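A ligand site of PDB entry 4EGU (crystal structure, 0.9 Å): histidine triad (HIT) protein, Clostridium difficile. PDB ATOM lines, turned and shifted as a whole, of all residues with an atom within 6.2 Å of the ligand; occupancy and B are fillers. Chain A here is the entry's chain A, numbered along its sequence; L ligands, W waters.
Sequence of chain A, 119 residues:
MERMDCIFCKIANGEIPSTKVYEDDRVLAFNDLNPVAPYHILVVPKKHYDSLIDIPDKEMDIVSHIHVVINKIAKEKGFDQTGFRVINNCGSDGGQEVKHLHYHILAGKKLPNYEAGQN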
ATOM      1  N   ILE A   7       1.669  24.713 -23.398  1.00  0.00           N
ATOM      2  CA  ILE A   7       1.814  23.602 -24.305  1.00  0.00           C
ATOM      3  C   ILE A   7       2.081  22.321 -23.491  1.00  0.00           C
ATOM      4  O   ILE A   7       1.561  21.261 -23.830  1.00  0.00           O
ATOM      5  CB  ILE A   7       2.960  23.841 -25.329  1.00  0.00           C
ATOM      6  CG1 ILE A   7       2.654  25.026 -26.251  1.00  0.00           C
ATOM      7  CG2 ILE A   7       3.230  22.578 -26.153  1.00  0.00           C
ATOM      8  CD1 ILE A   7       3.858  25.500 -27.037  1.00  0.00           C
ATOM      9  N   PHE A   8       2.906  22.395 -22.458  1.00  0.00           N
ATOM     10  CA  PHE A   8       3.272  21.170 -21.734  1.00  0.00           C
ATOM     11  C   PHE A   8       2.128  20.656 -20.842  1.00  0.00           C
ATOM     12  O   PHE A   8       2.034  19.444 -20.659  1.00  0.00           O
ATOM     13  CB  PHE A   8       4.581  21.323 -20.958  1.00  0.00           C
ATOM     14  CG  PHE A   8       5.820  21.421 -21.826  1.00  0.00           C
ATOM     15  CD1 PHE A   8       5.788  21.361 -23.216  1.00  0.00           C
ATOM     16  CD2 PHE A   8       7.056  21.593 -21.222  1.00  0.00           C
ATOM     17  CE1 PHE A   8       6.958  21.465 -23.980  1.00  0.00           C
ATOM     18  CE2 PHE A   8       8.210  21.694 -21.979  1.00  0.00           C
ATOM     19  CZ  PHE A   8       8.170  21.625 -23.360  1.00  0.00           C
ATOM     20  N   ILE A  11       0.263  18.708 -23.414  1.00  0.00           N
ATOM     21  CA  ILE A  11       0.980  17.475 -23.726  1.00  0.00           C
ATOM     22  C   ILE A  11       0.830  16.479 -22.540  1.00  0.00           C
ATOM     23  O   ILE A  11       0.573  15.303 -22.756  1.00  0.00           O
ATOM     24  CB  ILE A  11       2.466  17.736 -24.123  1.00  0.00           C
ATOM     25  CG1 ILE A  11       2.551  18.439 -25.482  1.00  0.00           C
ATOM     26  CG2 ILE A  11       3.259  16.429 -24.122  1.00  0.00           C
ATOM     27  CD1 ILE A  11       3.949  18.808 -25.936  1.00  0.00           C
ATOM     28  N   ILE A  16      -2.799  17.224 -26.414  1.00  0.00           N
ATOM     29  CA  ILE A  16      -1.958  17.443 -27.593  1.00  0.00           C
ATOM     30  C   ILE A  16      -1.083  16.213 -27.836  1.00  0.00           C
ATOM     31  O   ILE A  16      -0.540  15.670 -26.876  1.00  0.00           O
ATOM     32  CB  ILE A  16      -1.014  18.638 -27.357  1.00  0.00           C
ATOM     33  CG1 ILE A  16      -1.790  19.950 -27.395  1.00  0.00           C
ATOM     34  CG2 ILE A  16       0.119  18.644 -28.375  1.00  0.00           C
ATOM     35  CD1 ILE A  16      -3.013  19.882 -28.246  1.00  0.00           C
ATOM     36  N   PRO A  17      -0.907  15.783 -29.108  1.00  0.00           N
ATOM     37  CA  PRO A  17      -0.033  14.620 -29.347  1.00  0.00           C
ATOM     38  C   PRO A  17       1.450  14.865 -29.051  1.00  0.00           C
ATOM     39  O   PRO A  17       1.973  15.972 -29.219  1.00  0.00           O
ATOM     40  CB  PRO A  17      -0.206  14.324 -30.843  1.00  0.00           C
ATOM     41  CG  PRO A  17      -1.506  14.941 -31.211  1.00  0.00           C
ATOM     42  CD  PRO A  17      -1.643  16.163 -30.322  1.00  0.00           C
ATOM     43  N   SER A  18       2.114  13.797 -28.617  1.00  0.00           N
ATOM     44  CA  SER A  18       3.558  13.778 -28.457  1.00  0.00           C
ATOM     45  C   SER A  18       4.031  12.334 -28.615  1.00  0.00           C
ATOM     46  O   SER A  18       3.231  11.387 -28.629  1.00  0.00           O
ATOM     47  CB  SER A  18       3.947  14.297 -27.082  1.00  0.00           C
ATOM     48  OG  SER A  18       3.505  13.433 -26.050  1.00  0.00           O
ATOM     49  N   THR A  19       5.344  12.189 -28.725  1.00  0.00           N
ATOM     50  CA  THR A  19       5.969  10.872 -28.774  1.00  0.00           C
ATOM     51  C   THR A  19       6.498  10.555 -27.388  1.00  0.00           C
ATOM     52  O   THR A  19       7.517  11.092 -26.945  1.00  0.00           O
ATOM     53  CB  THR A  19       7.083  10.823 -29.825  1.00  0.00           C
ATOM     54  OG1 THR A  19       6.533  11.099 -31.119  1.00  0.00           O
ATOM     55  CG2 THR A  19       7.751   9.458 -29.836  1.00  0.00           C
ATOM     56  N   PHE A  30       8.846  12.895 -23.160  1.00  0.00           N
ATOM     57  CA  PHE A  30       8.481  12.841 -24.547  1.00  0.00           C
ATOM     58  C   PHE A  30       9.600  13.454 -25.382  1.00  0.00           C
ATOM     59  O   PHE A  30      10.407  14.225 -24.888  1.00  0.00           O
ATOM     60  CB  PHE A  30       7.101  13.537 -24.800  1.00  0.00           C
ATOM     61  CG  PHE A  30       7.016  14.975 -24.292  1.00  0.00           C
ATOM     62  CD1 PHE A  30       6.742  15.271 -22.954  1.00  0.00           C
ATOM     63  CD2 PHE A  30       7.264  16.031 -25.149  1.00  0.00           C
ATOM     64  CE1 PHE A  30       6.688  16.594 -22.510  1.00  0.00           C
ATOM     65  CE2 PHE A  30       7.197  17.351 -24.709  1.00  0.00           C
ATOM     66  CZ  PHE A  30       6.927  17.623 -23.388  1.00  0.00           C
ATOM     67  N   ASN A  31       9.666  13.106 -26.654  1.00  0.00           N
ATOM     68  CA  ASN A  31      10.725  13.660 -27.480  1.00  0.00           C
ATOM     69  C   ASN A  31      10.529  15.125 -27.764  1.00  0.00           C
ATOM     70  O   ASN A  31       9.402  15.582 -27.992  1.00  0.00           O
ATOM     71  CB  ASN A  31      10.800  12.900 -28.786  1.00  0.00           C
ATOM     72  CG  ASN A  31      11.316  11.488 -28.609  1.00  0.00           C
ATOM     73  OD1 ASN A  31      12.136  11.201 -27.724  1.00  0.00           O
ATOM     74  ND2 ASN A  31      10.874  10.619 -29.475  1.00  0.00           N
ATOM     75  N   ASP A  32      11.624  15.861 -27.798  1.00  0.00           N
ATOM     76  CA  ASP A  32      11.560  17.261 -28.151  1.00  0.00           C
ATOM     77  C   ASP A  32      11.177  17.359 -29.620  1.00  0.00           C
ATOM     78  O   ASP A  32      11.688  16.602 -30.425  1.00  0.00           O
ATOM     79  CB  ASP A  32      12.924  17.892 -27.926  1.00  0.00           C
ATOM     80  CG  ASP A  32      12.870  19.398 -27.938  1.00  0.00           C
ATOM     81  OD1 ASP A  32      12.700  19.967 -29.027  1.00  0.00           O
ATOM     82  OD2 ASP A  32      12.998  20.010 -26.862  1.00  0.00           O
ATOM     83  N   LEU A  33      10.295  18.308 -29.964  1.00  0.00           N
ATOM     84  CA  LEU A  33       9.875  18.522 -31.349  1.00  0.00           C
ATOM     85  C   LEU A  33      11.036  18.948 -32.259  1.00  0.00           C
ATOM     86  O   LEU A  33      11.012  18.676 -33.460  1.00  0.00           O
ATOM     87  CB  LEU A  33       8.785  19.593 -31.389  1.00  0.00           C
ATOM     88  CG  LEU A  33       8.194  19.942 -32.755  1.00  0.00           C
ATOM     89  CD1 LEU A  33       7.645  18.708 -33.455  1.00  0.00           C
ATOM     90  CD2 LEU A  33       7.121  20.975 -32.566  1.00  0.00           C
ATOM     91  N   ASN A  34      12.029  19.614 -31.678  1.00  0.00           N
ATOM     92  CA  ASN A  34      13.159  20.203 -32.413  1.00  0.00           C
ATOM     93  C   ASN A  34      14.466  19.678 -31.819  1.00  0.00           C
ATOM     94  O   ASN A  34      15.221  20.434 -31.204  1.00  0.00           O
ATOM     95  CB  ASN A  34      13.093  21.742 -32.338  1.00  0.00           C
ATOM     96  CG  ASN A  34      11.746  22.300 -32.799  1.00  0.00           C
ATOM     97  OD1 ASN A  34      10.943  22.803 -31.977  1.00  0.00           O
ATOM     98  ND2 ASN A  34      11.474  22.200 -34.081  1.00  0.00           N
ATOM     99  N   PRO A  35      14.758  18.380 -32.015  1.00  0.00           N
ATOM    100  CA  PRO A  35      15.890  17.790 -31.270  1.00  0.00           C
ATOM    101  C   PRO A  35      17.248  18.267 -31.673  1.00  0.00           C
ATOM    102  O   PRO A  35      17.519  18.472 -32.857  1.00  0.00           O
ATOM    103  CB  PRO A  35      15.746  16.288 -31.570  1.00  0.00           C
ATOM    104  CG  PRO A  35      15.017  16.242 -32.901  1.00  0.00           C
ATOM    105  CD  PRO A  35      14.027  17.376 -32.821  1.00  0.00           C
ATOM    106  N   HIS A  40      16.865  13.487 -27.580  1.00  0.00           N
ATOM    107  CA  HIS A  40      16.570  14.805 -27.009  1.00  0.00           C
ATOM    108  C   HIS A  40      15.181  14.671 -26.415  1.00  0.00           C
ATOM    109  O   HIS A  40      14.165  14.697 -27.127  1.00  0.00           O
ATOM    110  CB  HIS A  40      16.653  15.915 -28.027  1.00  0.00           C
ATOM    111  CG  HIS A  40      16.487  17.262 -27.399  1.00  0.00           C
ATOM    112  ND1 HIS A  40      16.699  18.427 -28.087  1.00  0.00           N
ATOM    113  CD2 HIS A  40      16.145  17.623 -26.139  1.00  0.00           C
ATOM    114  CE1 HIS A  40      16.481  19.448 -27.289  1.00  0.00           C
ATOM    115  NE2 HIS A  40      16.135  18.987 -26.094  1.00  0.00           N
ATOM    116  N   LEU A  42      12.359  15.471 -23.257  1.00  0.00           N
ATOM    117  CA  LEU A  42      11.875  16.391 -22.237  1.00  0.00           C
ATOM    118  C   LEU A  42      11.192  15.583 -21.147  1.00  0.00           C
ATOM    119  O   LEU A  42      10.337  14.753 -21.430  1.00  0.00           O
ATOM    120  CB  LEU A  42      10.858  17.363 -22.844  1.00  0.00           C
ATOM    121  CG  LEU A  42      11.465  18.340 -23.825  1.00  0.00           C
ATOM    122  CD1 LEU A  42      10.410  18.968 -24.728  1.00  0.00           C
ATOM    123  CD2 LEU A  42      12.148  19.451 -23.053  1.00  0.00           C
ATOM    124  N   ASN A  89      16.540  25.025 -17.876  1.00  0.00           N
ATOM    125  CA  ASN A  89      16.596  26.440 -18.204  1.00  0.00           C
ATOM    126  C   ASN A  89      15.552  27.170 -17.360  1.00  0.00           C
ATOM    127  O   ASN A  89      14.365  26.865 -17.434  1.00  0.00           O
ATOM    128  CB  ASN A  89      16.266  26.624 -19.686  1.00  0.00           C
ATOM    129  CG  ASN A  89      17.273  25.997 -20.603  1.00  0.00           C
ATOM    130  OD1 ASN A  89      18.455  25.889 -20.284  1.00  0.00           O
ATOM    131  ND2 ASN A  89      16.808  25.548 -21.755  1.00  0.00           N
ATOM    132  N   GLY A  95      17.332  30.980 -20.866  1.00  0.00           N
ATOM    133  CA  GLY A  95      16.835  30.488 -22.130  1.00  0.00           C
ATOM    134  C   GLY A  95      15.549  29.701 -22.045  1.00  0.00           C
ATOM    135  O   GLY A  95      15.197  29.016 -22.974  1.00  0.00           O
ATOM    136  N   GLN A  96      14.838  29.804 -20.928  1.00  0.00           N
ATOM    137  CA  GLN A  96      13.567  29.096 -20.793  1.00  0.00           C
ATOM    138  C   GLN A  96      12.584  29.799 -21.681  1.00  0.00           C
ATOM    139  O   GLN A  96      12.465  31.033 -21.700  1.00  0.00           O
ATOM    140  CB  GLN A  96      13.060  29.180 -19.371  1.00  0.00           C
ATOM    141  CG  GLN A  96      11.937  28.243 -19.034  1.00  0.00           C
ATOM    142  CD  GLN A  96      11.241  28.628 -17.717  1.00  0.00           C
ATOM    143  OE1 GLN A  96      11.300  29.765 -17.243  1.00  0.00           O
ATOM    144  NE2 GLN A  96      10.465  27.697 -17.201  1.00  0.00           N
ATOM    145  N   GLU A  97      11.885  28.980 -22.452  1.00  0.00           N
ATOM    146  CA  GLU A  97      10.835  29.470 -23.352  1.00  0.00           C
ATOM    147  C   GLU A  97       9.439  28.963 -22.885  1.00  0.00           C
ATOM    148  O   GLU A  97       8.518  29.744 -22.679  1.00  0.00           O
ATOM    149  CB  GLU A  97      11.134  29.021 -24.795  1.00  0.00           C
ATOM    150  CG  GLU A  97      12.516  29.449 -25.312  1.00  0.00           C
ATOM    151  CD  GLU A  97      12.932  28.708 -26.568  1.00  0.00           C
ATOM    152  OE1 GLU A  97      13.231  27.487 -26.495  1.00  0.00           O
ATOM    153  OE2 GLU A  97      12.941  29.338 -27.628  1.00  0.00           O
ATOM    154  N   VAL A  98       9.336  27.655 -22.727  1.00  0.00           N
ATOM    155  CA  VAL A  98       8.089  27.045 -22.237  1.00  0.00           C
ATOM    156  C   VAL A  98       8.118  27.075 -20.719  1.00  0.00           C
ATOM    157  O   VAL A  98       8.977  26.435 -20.095  1.00  0.00           O
ATOM    158  CB  VAL A  98       7.888  25.622 -22.729  1.00  0.00           C
ATOM    159  CG1 VAL A  98       6.619  25.040 -22.163  1.00  0.00           C
ATOM    160  CG2 VAL A  98       7.856  25.595 -24.268  1.00  0.00           C
ATOM    161  N   LYS A  99       7.178  27.816 -20.149  1.00  0.00           N
ATOM    162  CA  LYS A  99       7.174  28.098 -18.716  1.00  0.00           C
ATOM    163  C   LYS A  99       6.369  27.028 -17.965  1.00  0.00           C
ATOM    164  O   LYS A  99       5.367  27.318 -17.290  1.00  0.00           O
ATOM    165  CB  LYS A  99       6.670  29.527 -18.461  1.00  0.00           C
ATOM    166  CG  LYS A  99       7.616  30.597 -19.000  1.00  0.00           C
ATOM    167  CD  LYS A  99       7.069  31.992 -18.745  1.00  0.00           C
ATOM    168  CE  LYS A  99       7.947  33.079 -19.338  1.00  0.00           C
ATOM    169  NZ  LYS A  99       7.390  34.448 -19.094  1.00  0.00           N
ATOM    170  N   HIS A 102      10.636  21.652 -16.825  1.00  0.00           N
ATOM    171  CA  HIS A 102      11.069  20.554 -17.677  1.00  0.00           C
ATOM    172  C   HIS A 102      12.558  20.417 -17.629  1.00  0.00           C
ATOM    173  O   HIS A 102      13.289  21.403 -17.492  1.00  0.00           O
ATOM    174  CB  HIS A 102      10.615  20.816 -19.161  1.00  0.00           C
ATOM    175  CG  HIS A 102      11.156  22.084 -19.769  1.00  0.00           C
ATOM    176  ND1 HIS A 102      10.521  23.281 -19.575  1.00  0.00           N
ATOM    177  CD2 HIS A 102      12.235  22.362 -20.544  1.00  0.00           C
ATOM    178  CE1 HIS A 102      11.178  24.250 -20.205  1.00  0.00           C
ATOM    179  NE2 HIS A 102      12.216  23.708 -20.805  1.00  0.00           N
ATOM    180  N   HIS A 104      15.707  18.778 -19.952  1.00  0.00           N
ATOM    181  CA  HIS A 104      16.195  18.214 -21.201  1.00  0.00           C
ATOM    182  C   HIS A 104      17.208  17.120 -20.910  1.00  0.00           C
ATOM    183  O   HIS A 104      18.119  17.325 -20.114  1.00  0.00           O
ATOM    184  CB  HIS A 104      16.923  19.264 -22.037  1.00  0.00           C
ATOM    185  CG  HIS A 104      16.113  20.462 -22.432  1.00  0.00           C
ATOM    186  ND1 HIS A 104      15.584  20.577 -23.696  1.00  0.00           N
ATOM    187  CD2 HIS A 104      15.854  21.618 -21.774  1.00  0.00           C
ATOM    188  CE1 HIS A 104      14.969  21.750 -23.767  1.00  0.00           C
ATOM    189  NE2 HIS A 104      15.127  22.397 -22.621  1.00  0.00           N
HETATM  190  P1  LIG L   1      13.112  25.571 -23.402  1.00  0.00           P
HETATM  191  O1  LIG L   1      13.974  26.333 -24.392  1.00  0.00           O
HETATM  192  O2  LIG L   1      11.876  26.284 -22.920  1.00  0.00           O
HETATM  193  O3  LIG L   1      13.917  25.115 -22.266  1.00  0.00           O
HETATM  194  O4  LIG L   1      12.721  24.194 -24.062  1.00  0.00           O
HETATM  195  C1  LIG L   1      11.437  24.011 -24.617  1.00  0.00           C
HETATM  196  C2  LIG L   1      11.489  22.923 -25.629  1.00  0.00           C
HETATM  197  O5  LIG L   1      10.150  22.561 -25.975  1.00  0.00           O
HETATM  198  C3  LIG L   1      12.197  23.302 -26.925  1.00  0.00           C
HETATM  199  O6  LIG L   1      13.387  22.521 -27.080  1.00  0.00           O
HETATM  200  C4  LIG L   1      11.166  22.945 -28.028  1.00  0.00           C
HETATM  201  O7  LIG L   1      11.696  22.306 -29.173  1.00  0.00           O
HETATM  202  C5  LIG L   1      10.163  22.060 -27.270  1.00  0.00           C
HETATM  203  N1  LIG L   1       8.795  22.122 -27.778  1.00  0.00           N
HETATM  204  C6  LIG L   1       8.099  23.255 -27.955  1.00  0.00           C
HETATM  205  N2  LIG L   1       6.849  22.976 -28.386  1.00  0.00           N
HETATM  206  C7  LIG L   1       6.769  21.628 -28.460  1.00  0.00           C
HETATM  207  C8  LIG L   1       5.733  20.777 -28.838  1.00  0.00           C
HETATM  208  O8  LIG L   1       4.597  21.183 -29.222  1.00  0.00           O
HETATM  209  N3  LIG L   1       6.023  19.471 -28.771  1.00  0.00           N
HETATM  210  C9  LIG L   1       7.226  18.982 -28.370  1.00  0.00           C
HETATM  211  N4  LIG L   1       7.385  17.648 -28.350  1.00  0.00           N
HETATM  212  N5  LIG L   1       8.254  19.770 -27.999  1.00  0.00           N
HETATM  213  C10 LIG L   1       7.995  21.093 -28.058  1.00  0.00           C
HETATM  214  O   HOH W   1      15.197  22.404 -29.286  1.00  0.00           O
HETATM  215  O   HOH W   2      15.296  24.499 -26.271  1.00  0.00           O
HETATM  216  O   HOH W   3      16.672  27.962 -25.137  1.00  0.00           O
HETATM  217  O   HOH W   4       4.510  17.113 -29.435  1.00  0.00           O
HETATM  218  O   HOH W   5       7.054  14.448 -28.904  1.00  0.00           O
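An oxygen (O3) of the ligand lies within hydrogen-bond range of the side-chain amide nitrogen (ND2) of Asn 89 (3.0 Å).
A ring nitrogen (NE2) of His 104 sits at hydrogen-bond distance from an oxygen (O3) of the ligand, at 3.0 Å.
An oxygen (O2) of the ligand sits at hydrogen-bond distance from the backbone NH of Val 98 (2.9 Å).
O3 of the ligand lies within hydrogen-bond range of NE2 of His 102.
A nitrogen (N5) of the ligand is in hydrogen-bond range of the backbone NH (N) of Leu 33 (3.2 Å).
OD1 of Asn 34 sits at hydrogen-bond distance from O7 of the ligand (2.9 Å).
O2 of the ligand sits at hydrogen-bond distance from N of Glu 97, at 2.7 Å.
The side-chain carboxylate (OE1) of Glu 97 lies close to an oxygen (O1) of the ligand (2.5 Å).
The side-chain carboxylate of Asp 32 is in hydrogen-bond range of an oxygen (O7) of the ligand, 2.5 Å away.
O of Asn 31 sits at hydrogen-bond distance from N4 of the ligand (2.9 Å).
O of Phe 30 is in hydrogen-bond range of N of Leu 42, 2.8 Å away.
OD1 of Asp 32 is in hydrogen-bond range of N of Asn 34 (2.8 Å).
The backbone carbonyl oxygen of Val 98 lies within hydrogen-bond range of the side-chain amide nitrogen of Gln 96, at 3.5 Å.
ND1 of His 104 is in hydrogen-bond range of NE2 of His 40, at 2.9 Å.
N of Asp 32 lies within hydrogen-bond range of O of His 40, 2.9 Å away.
The backbone NH of Asn 31 lies within hydrogen-bond range of the backbone carbonyl oxygen of Thr 19 (3.0 Å).
O of Gly 95 lies close to O1 of the ligand, 3.3 Å away.
Merely in contact with the ligand: Ile 7 (3.6 Å), Phe 8 (3.4 Å), Ile 11 (3.6 Å), Phe 30 (3.6 Å), Leu 42 (3.8 Å) and Gln 96 (3.8 Å).
16 residues have an atom within 4 Å of the ligand: Ile 7, Phe 8, Ile 11, Phe 30, Asn 31, Asp 32, Leu 33, Asn 34, Leu 42, Asn 89, Gly 95, Gln 96, Glu 97, Val 98, His 102 and His 104.
Water W1 lies within hydrogen-bond range of O of Asn 34 (2.7 Å), O6 of the ligand (2.9 Å) and OD1 of Asp 32 (3.5 Å).
Water W4 lies within hydrogen-bond range of the backbone carbonyl oxygen of Pro 17 (2.8 Å) and a nitrogen (N3) of the ligand (2.9 Å).
Water W3 lies within hydrogen-bond range of O of Gly 95 and O1 of the ligand.
Water W5 lies within hydrogen-bond range of O of Asn 31, N of Thr 19 and N4 of the ligand.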
